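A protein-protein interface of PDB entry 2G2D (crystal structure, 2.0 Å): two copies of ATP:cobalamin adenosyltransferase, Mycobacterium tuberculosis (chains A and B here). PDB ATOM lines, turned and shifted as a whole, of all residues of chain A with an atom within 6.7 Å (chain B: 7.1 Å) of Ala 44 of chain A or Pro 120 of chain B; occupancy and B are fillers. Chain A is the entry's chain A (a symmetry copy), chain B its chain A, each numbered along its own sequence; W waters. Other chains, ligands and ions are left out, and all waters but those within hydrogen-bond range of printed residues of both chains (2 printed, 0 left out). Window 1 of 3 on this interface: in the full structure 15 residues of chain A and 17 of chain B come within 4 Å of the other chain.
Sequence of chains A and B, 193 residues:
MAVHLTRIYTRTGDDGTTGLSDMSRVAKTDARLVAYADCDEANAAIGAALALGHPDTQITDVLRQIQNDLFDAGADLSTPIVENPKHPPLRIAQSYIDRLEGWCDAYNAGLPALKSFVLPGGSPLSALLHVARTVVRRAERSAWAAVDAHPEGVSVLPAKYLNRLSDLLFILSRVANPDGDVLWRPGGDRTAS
The side-chain amide nitrogen of Gln 67 of chain A sits at hydrogen-bond distance from the backbone carbonyl oxygen of Pro 120 of chain B, at 3.0 Å.
NH1 of Arg 133 of chain B lies within salt-bridge range of OD2 of Asp 40 of chain A.
Of the printed residues of chain B, Ala 44 of chain A touches Pro 120, His 130, Val 131 and Thr 134.
Pro 120 of chain B touches just these residues of chain A: Asn 43 (3.6 Å), Ala 44 (3.5 Å), Gly 47 (3.4 Å) and Gln 67 (3.0 Å).
Printed residues of chain A within 4 Å of Thr 134 of chain B: Asp 40, Glu 41 and Ala 44.
Of the printed residues of chain A, His 130 of chain B touches Ala 44.
Printed residues of chain B within 4 Å of Phe 71 of chain A: Leu 119.
Leu 129 of chain B touches none of the printed residues of chain A.
Ala 49 of chain A touches none of the printed residues of chain B.
The nearest printed residue of chain B that does not touch Ala 44 of chain A is Ala 127 of chain B (4.7 Å).
The nearest printed residue of chain A that does not touch Val 131 of chain B is Ala 48 of chain A (4.2 Å).
Water W1 bridges the backbone carbonyl oxygen (O) of Ala 44 of chain A (2.8 Å) and the backbone carbonyl oxygen (O) of Ala 127 of chain B (2.9 Å).
Water W2 bridges the backbone NH (N) of Gly 122 of chain B (2.8 Å) and the backbone carbonyl oxygen (O) of Gly 47 of chain A (2.9 Å).
Of the 15 printed residues of chain A, 7 touch a printed residue of chain B.
Printed residues of chain A that touch a printed residue of chain B: Asp 40, Glu 41, Asn 43, Ala 44, Gly 47, Gln 67 and Phe 71.
Among the printed residues, 13 pairs touch across the chains.
N of Leu 119 of chain B is in hydrogen-bond range of O of Val 182 of chain B (2.7 Å).
The backbone carbonyl oxygen of Val 131 of chain B sits at hydrogen-bond distance from the side-chain hydroxyl of Thr 134 of chain B.
The backbone carbonyl oxygen of Asn 43 of chain A is in hydrogen-bond range of the side-chain amide nitrogen of Gln 67 of chain A (3.1 Å).
The backbone carbonyl oxygen (O) of Ser 126 of chain B is in hydrogen-bond range of a ring nitrogen (ND1) of His 130 of chain B (3.3 Å).
N of Gly 47 of chain A sits close to NE2 of Gln 67 of chain A.
Glu 41 of chain A touches Thr 134 of chain B.
Asn 43 of chain A touches Pro 120 of chain B.
Pro 120 of chain B touches Ala 44 of chain A.
Ala 44 of chain A touches His 130 of chain B.
O of Ala 44 of chain A touches CG2 of Val 131 of chain B, at 3.6 Å.
Ala 44 of chain A touches Thr 134 of chain B.
Gly 47 of chain A touches Pro 120 of chain B (CA to O, 3.4 Å).
Gly 47 of chain A touches Ala 127 of chain B (O to CB, 3.8 Å).
Gln 67 of chain A touches Leu 119 of chain B (O to CD2, 3.9 Å).
CD2 of Leu 119 of chain B touches CB of Phe 71 of chain A, at 3.8 Å.
No position is printed for both chains.
Of the 13 pairs that touch across the chains among the printed residues, none has its exchanged pair printed and touching as well.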
ATOM      1  N   CYS A  39      -0.158  -2.306  16.662  1.00  0.00           N
ATOM      2  CA  CYS A  39      -1.540  -1.815  16.742  1.00  0.00           C
ATOM      3  C   CYS A  39      -2.434  -2.729  15.929  1.00  0.00           C
ATOM      4  O   CYS A  39      -3.568  -3.021  16.321  1.00  0.00           O
ATOM      5  CB  CYS A  39      -1.678  -0.399  16.166  1.00  0.00           C
ATOM      6  SG  CYS A  39      -1.512   0.910  17.386  1.00  0.00           S
ATOM      7  N   ASP A  40      -1.908  -3.160  14.785  1.00  0.00           N
ATOM      8  CA  ASP A  40      -2.625  -4.057  13.880  1.00  0.00           C
ATOM      9  C   ASP A  40      -2.825  -5.417  14.602  1.00  0.00           C
ATOM     10  O   ASP A  40      -3.910  -6.011  14.534  1.00  0.00           O
ATOM     11  CB  ASP A  40      -1.813  -4.189  12.583  1.00  0.00           C
ATOM     12  CG  ASP A  40      -2.479  -5.087  11.545  1.00  0.00           C
ATOM     13  OD1 ASP A  40      -3.706  -5.313  11.617  1.00  0.00           O
ATOM     14  OD2 ASP A  40      -1.761  -5.558  10.643  1.00  0.00           O
ATOM     15  N   GLU A  41      -1.797  -5.890  15.312  1.00  0.00           N
ATOM     16  CA  GLU A  41      -1.912  -7.161  16.053  1.00  0.00           C
ATOM     17  C   GLU A  41      -2.975  -7.014  17.150  1.00  0.00           C
ATOM     18  O   GLU A  41      -3.787  -7.912  17.363  1.00  0.00           O
ATOM     19  CB  GLU A  41      -0.563  -7.566  16.681  1.00  0.00           C
ATOM     20  CG  GLU A  41      -0.526  -9.025  17.189  1.00  0.00           C
ATOM     21  CD  GLU A  41       0.861  -9.488  17.655  1.00  0.00           C
ATOM     22  OE1 GLU A  41       1.864  -8.793  17.387  1.00  0.00           O
ATOM     23  OE2 GLU A  41       0.948 -10.570  18.279  1.00  0.00           O
ATOM     24  N   ALA A  42      -2.973  -5.884  17.853  1.00  0.00           N
ATOM     25  CA  ALA A  42      -3.989  -5.651  18.885  1.00  0.00           C
ATOM     26  C   ALA A  42      -5.370  -5.588  18.230  1.00  0.00           C
ATOM     27  O   ALA A  42      -6.348  -6.127  18.755  1.00  0.00           O
ATOM     28  CB  ALA A  42      -3.718  -4.347  19.621  1.00  0.00           C
ATOM     29  N   ASN A  43      -5.456  -4.931  17.077  1.00  0.00           N
ATOM     30  CA  ASN A  43      -6.741  -4.833  16.397  1.00  0.00           C
ATOM     31  C   ASN A  43      -7.262  -6.219  16.016  1.00  0.00           C
ATOM     32  O   ASN A  43      -8.463  -6.492  16.151  1.00  0.00           O
ATOM     33  CB  ASN A  43      -6.630  -3.936  15.154  1.00  0.00           C
ATOM     34  CG  ASN A  43      -7.952  -3.269  14.796  1.00  0.00           C
ATOM     35  OD1 ASN A  43      -8.981  -3.557  15.402  1.00  0.00           O
ATOM     36  ND2 ASN A  43      -7.928  -2.369  13.806  1.00  0.00           N
ATOM     37  N   ALA A  44      -6.373  -7.105  15.557  1.00  0.00           N
ATOM     38  CA  ALA A  44      -6.796  -8.459  15.186  1.00  0.00           C
ATOM     39  C   ALA A  44      -7.262  -9.243  16.415  1.00  0.00           C
ATOM     40  O   ALA A  44      -8.173 -10.079  16.316  1.00  0.00           O
ATOM     41  CB  ALA A  44      -5.648  -9.226  14.458  1.00  0.00           C
ATOM     42  N   ALA A  45      -6.643  -8.994  17.572  1.00  0.00           N
ATOM     43  CA  ALA A  45      -7.082  -9.672  18.804  1.00  0.00           C
ATOM     44  C   ALA A  45      -8.526  -9.234  19.143  1.00  0.00           C
ATOM     45  O   ALA A  45      -9.331 -10.036  19.617  1.00  0.00           O
ATOM     46  CB  ALA A  45      -6.131  -9.345  19.971  1.00  0.00           C
ATOM     47  N   ILE A  46      -8.863  -7.966  18.908  1.00  0.00           N
ATOM     48  CA  ILE A  46     -10.245  -7.512  19.166  1.00  0.00           C
ATOM     49  C   ILE A  46     -11.179  -8.210  18.162  1.00  0.00           C
ATOM     50  O   ILE A  46     -12.287  -8.651  18.514  1.00  0.00           O
ATOM     51  CB  ILE A  46     -10.364  -5.960  19.048  1.00  0.00           C
ATOM     52  CG1 ILE A  46      -9.547  -5.311  20.179  1.00  0.00           C
ATOM     53  CG2 ILE A  46     -11.841  -5.526  19.176  1.00  0.00           C
ATOM     54  CD1 ILE A  46      -9.575  -3.817  20.172  1.00  0.00           C
ATOM     55  N   GLY A  47     -10.721  -8.342  16.918  1.00  0.00           N
ATOM     56  CA  GLY A  47     -11.517  -9.043  15.919  1.00  0.00           C
ATOM     57  C   GLY A  47     -11.823 -10.487  16.349  1.00  0.00           C
ATOM     58  O   GLY A  47     -12.918 -10.995  16.105  1.00  0.00           O
ATOM     59  N   ALA A  48     -10.866 -11.155  16.988  1.00  0.00           N
ATOM     60  CA  ALA A  48     -11.083 -12.534  17.436  1.00  0.00           C
ATOM     61  C   ALA A  48     -12.120 -12.557  18.555  1.00  0.00           C
ATOM     62  O   ALA A  48     -12.979 -13.431  18.604  1.00  0.00           O
ATOM     63  CB  ALA A  48      -9.781 -13.147  17.918  1.00  0.00           C
ATOM     64  N   ALA A  49     -12.039 -11.585  19.456  1.00  0.00           N
ATOM     65  CA  ALA A  49     -12.991 -11.483  20.556  1.00  0.00           C
ATOM     66  C   ALA A  49     -14.405 -11.341  19.997  1.00  0.00           C
ATOM     67  O   ALA A  49     -15.342 -12.009  20.449  1.00  0.00           O
ATOM     68  CB  ALA A  49     -12.648 -10.285  21.418  1.00  0.00           C
ATOM     69  N   LEU A  50     -14.559 -10.467  19.008  1.00  0.00           N
ATOM     70  CA  LEU A  50     -15.866 -10.249  18.391  1.00  0.00           C
ATOM     71  C   LEU A  50     -16.367 -11.480  17.646  1.00  0.00           C
ATOM     72  O   LEU A  50     -17.550 -11.815  17.705  1.00  0.00           O
ATOM     73  CB  LEU A  50     -15.799  -9.081  17.399  1.00  0.00           C
ATOM     74  CG  LEU A  50     -15.747  -7.646  17.928  1.00  0.00           C
ATOM     75  CD1 LEU A  50     -15.160  -6.700  16.873  1.00  0.00           C
ATOM     76  CD2 LEU A  50     -17.152  -7.214  18.287  1.00  0.00           C
ATOM     77  N   GLN A  67     -12.117  -0.881  16.998  1.00  0.00           N
ATOM     78  CA  GLN A  67     -11.355  -1.397  15.840  1.00  0.00           C
ATOM     79  C   GLN A  67     -11.111  -0.251  14.865  1.00  0.00           C
ATOM     80  O   GLN A  67     -10.029  -0.116  14.296  1.00  0.00           O
ATOM     81  CB  GLN A  67     -12.119  -2.515  15.134  1.00  0.00           C
ATOM     82  CG  GLN A  67     -12.184  -3.813  15.936  1.00  0.00           C
ATOM     83  CD  GLN A  67     -12.266  -5.037  15.039  1.00  0.00           C
ATOM     84  OE1 GLN A  67     -13.301  -5.316  14.454  1.00  0.00           O
ATOM     85  NE2 GLN A  67     -11.158  -5.765  14.920  1.00  0.00           N
ATOM     86  N   LEU A  70      -8.396   1.966  16.310  1.00  0.00           N
ATOM     87  CA  LEU A  70      -7.066   1.358  16.211  1.00  0.00           C
ATOM     88  C   LEU A  70      -6.468   1.510  14.801  1.00  0.00           C
ATOM     89  O   LEU A  70      -5.245   1.588  14.637  1.00  0.00           O
ATOM     90  CB  LEU A  70      -7.115  -0.120  16.643  1.00  0.00           C
ATOM     91  CG  LEU A  70      -7.240  -0.315  18.168  1.00  0.00           C
ATOM     92  CD1 LEU A  70      -7.391  -1.775  18.507  1.00  0.00           C
ATOM     93  CD2 LEU A  70      -5.995   0.250  18.877  1.00  0.00           C
ATOM     94  N   PHE A  71      -7.325   1.552  13.787  1.00  0.00           N
ATOM     95  CA  PHE A  71      -6.847   1.757  12.411  1.00  0.00           C
ATOM     96  C   PHE A  71      -6.251   3.167  12.386  1.00  0.00           C
ATOM     97  O   PHE A  71      -5.143   3.399  11.894  1.00  0.00           O
ATOM     98  CB  PHE A  71      -8.013   1.691  11.426  1.00  0.00           C
ATOM     99  CG  PHE A  71      -7.607   1.925   9.995  1.00  0.00           C
ATOM    100  CD1 PHE A  71      -7.190   0.872   9.194  1.00  0.00           C
ATOM    101  CD2 PHE A  71      -7.611   3.217   9.464  1.00  0.00           C
ATOM    102  CE1 PHE A  71      -6.780   1.097   7.885  1.00  0.00           C
ATOM    103  CE2 PHE A  71      -7.201   3.458   8.154  1.00  0.00           C
ATOM    104  CZ  PHE A  71      -6.783   2.398   7.362  1.00  0.00           C
ATOM    105  N   VAL B 118      -9.693  -2.580   5.089  1.00  0.00           N
ATOM    106  CA  VAL B 118     -10.214  -3.713   5.850  1.00  0.00           C
ATOM    107  C   VAL B 118      -9.791  -3.709   7.322  1.00  0.00           C
ATOM    108  O   VAL B 118      -8.621  -3.479   7.637  1.00  0.00           O
ATOM    109  CB  VAL B 118      -9.729  -5.044   5.196  1.00  0.00           C
ATOM    110  CG1 VAL B 118     -10.049  -6.243   6.087  1.00  0.00           C
ATOM    111  CG2 VAL B 118     -10.381  -5.202   3.834  1.00  0.00           C
ATOM    112  N   LEU B 119     -10.742  -3.947   8.223  1.00  0.00           N
ATOM    113  CA  LEU B 119     -10.406  -4.040   9.640  1.00  0.00           C
ATOM    114  C   LEU B 119     -10.314  -5.551   9.876  1.00  0.00           C
ATOM    115  O   LEU B 119     -11.063  -6.314   9.276  1.00  0.00           O
ATOM    116  CB  LEU B 119     -11.492  -3.397  10.512  1.00  0.00           C
ATOM    117  CG  LEU B 119     -11.651  -1.876  10.335  1.00  0.00           C
ATOM    118  CD1 LEU B 119     -12.689  -1.336  11.332  1.00  0.00           C
ATOM    119  CD2 LEU B 119     -10.295  -1.188  10.550  1.00  0.00           C
ATOM    120  N   PRO B 120      -9.387  -6.002  10.736  1.00  0.00           N
ATOM    121  CA  PRO B 120      -9.262  -7.444  10.976  1.00  0.00           C
ATOM    122  C   PRO B 120     -10.424  -8.127  11.696  1.00  0.00           C
ATOM    123  O   PRO B 120     -10.738  -7.799  12.824  1.00  0.00           O
ATOM    124  CB  PRO B 120      -7.950  -7.556  11.751  1.00  0.00           C
ATOM    125  CG  PRO B 120      -7.854  -6.255  12.470  1.00  0.00           C
ATOM    126  CD  PRO B 120      -8.336  -5.249  11.446  1.00  0.00           C
ATOM    127  N   GLY B 121     -11.048  -9.095  11.039  1.00  0.00           N
ATOM    128  CA  GLY B 121     -12.148  -9.799  11.673  1.00  0.00           C
ATOM    129  C   GLY B 121     -13.165 -10.312  10.674  1.00  0.00           C
ATOM    130  O   GLY B 121     -12.878 -10.394   9.480  1.00  0.00           O
ATOM    131  N   GLY B 122     -14.360 -10.642  11.167  1.00  0.00           N
ATOM    132  CA  GLY B 122     -15.423 -11.149  10.319  1.00  0.00           C
ATOM    133  C   GLY B 122     -15.797 -12.531  10.826  1.00  0.00           C
ATOM    134  O   GLY B 122     -16.138 -12.697  11.996  1.00  0.00           O
ATOM    135  N   SER B 126     -11.817 -16.008   9.233  1.00  0.00           N
ATOM    136  CA  SER B 126     -11.167 -14.775   8.781  1.00  0.00           C
ATOM    137  C   SER B 126     -10.481 -14.076   9.944  1.00  0.00           C
ATOM    138  O   SER B 126      -9.359 -13.581   9.814  1.00  0.00           O
ATOM    139  CB  SER B 126     -12.186 -13.817   8.159  1.00  0.00           C
ATOM    140  OG  SER B 126     -12.832 -14.424   7.059  1.00  0.00           O
ATOM    141  N   ALA B 127     -11.158 -14.032  11.087  1.00  0.00           N
ATOM    142  CA  ALA B 127     -10.584 -13.389  12.274  1.00  0.00           C
ATOM    143  C   ALA B 127      -9.297 -14.099  12.704  1.00  0.00           C
ATOM    144  O   ALA B 127      -8.295 -13.450  13.021  1.00  0.00           O
ATOM    145  CB  ALA B 127     -11.591 -13.397  13.420  1.00  0.00           C
ATOM    146  N   LEU B 128      -9.334 -15.428  12.716  1.00  0.00           N
ATOM    147  CA  LEU B 128      -8.165 -16.230  13.110  1.00  0.00           C
ATOM    148  C   LEU B 128      -7.021 -16.123  12.089  1.00  0.00           C
ATOM    149  O   LEU B 128      -5.846 -16.215  12.447  1.00  0.00           O
ATOM    150  CB  LEU B 128      -8.583 -17.688  13.307  1.00  0.00           C
ATOM    151  CG  LEU B 128      -9.544 -17.915  14.488  1.00  0.00           C
ATOM    152  CD1 LEU B 128     -10.188 -19.294  14.397  1.00  0.00           C
ATOM    153  CD2 LEU B 128      -8.802 -17.754  15.791  1.00  0.00           C
ATOM    154  N   LEU B 129      -7.359 -15.929  10.817  1.00  0.00           N
ATOM    155  CA  LEU B 129      -6.323 -15.762   9.791  1.00  0.00           C
ATOM    156  C   LEU B 129      -5.698 -14.365   9.918  1.00  0.00           C
ATOM    157  O   LEU B 129      -4.510 -14.179   9.662  1.00  0.00           O
ATOM    158  CB  LEU B 129      -6.918 -15.986   8.390  1.00  0.00           C
ATOM    159  CG  LEU B 129      -7.207 -17.474   8.087  1.00  0.00           C
ATOM    160  CD1 LEU B 129      -7.991 -17.636   6.786  1.00  0.00           C
ATOM    161  CD2 LEU B 129      -5.879 -18.244   8.006  1.00  0.00           C
ATOM    162  N   HIS B 130      -6.493 -13.374  10.311  1.00  0.00           N
ATOM    163  CA  HIS B 130      -5.946 -12.038  10.518  1.00  0.00           C
ATOM    164  C   HIS B 130      -4.991 -12.094  11.722  1.00  0.00           C
ATOM    165  O   HIS B 130      -3.917 -11.470  11.717  1.00  0.00           O
ATOM    166  CB  HIS B 130      -7.064 -11.017  10.785  1.00  0.00           C
ATOM    167  CG  HIS B 130      -7.486 -10.260   9.561  1.00  0.00           C
ATOM    168  ND1 HIS B 130      -8.667 -10.513   8.895  1.00  0.00           N
ATOM    169  CD2 HIS B 130      -6.862  -9.280   8.864  1.00  0.00           C
ATOM    170  CE1 HIS B 130      -8.752  -9.722   7.842  1.00  0.00           C
ATOM    171  NE2 HIS B 130      -7.670  -8.966   7.797  1.00  0.00           N
ATOM    172  N   VAL B 131      -5.365 -12.841  12.759  1.00  0.00           N
ATOM    173  CA  VAL B 131      -4.455 -12.950  13.902  1.00  0.00           C
ATOM    174  C   VAL B 131      -3.143 -13.563  13.404  1.00  0.00           C
ATOM    175  O   VAL B 131      -2.069 -13.030  13.664  1.00  0.00           O
ATOM    176  CB  VAL B 131      -5.031 -13.832  15.038  1.00  0.00           C
ATOM    177  CG1 VAL B 131      -3.903 -14.211  16.042  1.00  0.00           C
ATOM    178  CG2 VAL B 131      -6.144 -13.063  15.780  1.00  0.00           C
ATOM    179  N   ALA B 132      -3.221 -14.676  12.672  1.00  0.00           N
ATOM    180  CA  ALA B 132      -1.990 -15.310  12.177  1.00  0.00           C
ATOM    181  C   ALA B 132      -1.225 -14.334  11.296  1.00  0.00           C
ATOM    182  O   ALA B 132       0.009 -14.260  11.357  1.00  0.00           O
ATOM    183  CB  ALA B 132      -2.316 -16.580  11.368  1.00  0.00           C
ATOM    184  N   ARG B 133      -1.956 -13.598  10.460  1.00  0.00           N
ATOM    185  CA  ARG B 133      -1.318 -12.630   9.571  1.00  0.00           C
ATOM    186  C   ARG B 133      -0.434 -11.664  10.350  1.00  0.00           C
ATOM    187  O   ARG B 133       0.721 -11.433   9.984  1.00  0.00           O
ATOM    188  CB  ARG B 133      -2.362 -11.819   8.784  1.00  0.00           C
ATOM    189  CG  ARG B 133      -1.740 -10.682   7.935  1.00  0.00           C
ATOM    190  CD  ARG B 133      -2.806  -9.876   7.147  1.00  0.00           C
ATOM    191  NE  ARG B 133      -3.808  -9.282   8.031  1.00  0.00           N
ATOM    192  CZ  ARG B 133      -3.597  -8.219   8.808  1.00  0.00           C
ATOM    193  NH1 ARG B 133      -2.416  -7.599   8.808  1.00  0.00           N
ATOM    194  NH2 ARG B 133      -4.554  -7.800   9.619  1.00  0.00           N
ATOM    195  N   THR B 134      -0.965 -11.097  11.433  1.00  0.00           N
ATOM    196  CA  THR B 134      -0.182 -10.128  12.183  1.00  0.00           C
ATOM    197  C   THR B 134       0.999 -10.781  12.874  1.00  0.00           C
ATOM    198  O   THR B 134       2.032 -10.163  13.015  1.00  0.00           O
ATOM    199  CB  THR B 134      -1.055  -9.380  13.215  1.00  0.00           C
ATOM    200  OG1 THR B 134      -1.565 -10.301  14.185  1.00  0.00           O
ATOM    201  CG2 THR B 134      -2.223  -8.684  12.479  1.00  0.00           C
ATOM    202  N   ASN B 177     -14.417 -14.637   4.184  1.00  0.00           N
ATOM    203  CA  ASN B 177     -15.503 -13.710   4.541  1.00  0.00           C
ATOM    204  C   ASN B 177     -16.398 -13.592   3.306  1.00  0.00           C
ATOM    205  O   ASN B 177     -16.357 -12.592   2.582  1.00  0.00           O
ATOM    206  CB  ASN B 177     -14.974 -12.311   4.892  1.00  0.00           C
ATOM    207  CG  ASN B 177     -14.687 -12.142   6.376  1.00  0.00           C
ATOM    208  OD1 ASN B 177     -15.343 -12.750   7.220  1.00  0.00           O
ATOM    209  ND2 ASN B 177     -13.721 -11.303   6.697  1.00  0.00           N
ATOM    210  N   VAL B 182     -14.887  -6.544   7.116  1.00  0.00           N
ATOM    211  CA  VAL B 182     -15.239  -5.509   8.084  1.00  0.00           C
ATOM    212  C   VAL B 182     -14.475  -4.297   7.566  1.00  0.00           C
ATOM    213  O   VAL B 182     -13.258  -4.364   7.419  1.00  0.00           O
ATOM    214  CB  VAL B 182     -14.748  -5.874   9.499  1.00  0.00           C
ATOM    215  CG1 VAL B 182     -15.152  -4.773  10.490  1.00  0.00           C
ATOM    216  CG2 VAL B 182     -15.366  -7.225   9.930  1.00  0.00           C
HETATM  217  O   HOH W   1      -9.118 -10.842  13.846  1.00  0.00           O
HETATM  218  O   HOH W   2     -14.587 -10.104  13.919  1.00  0.00           O
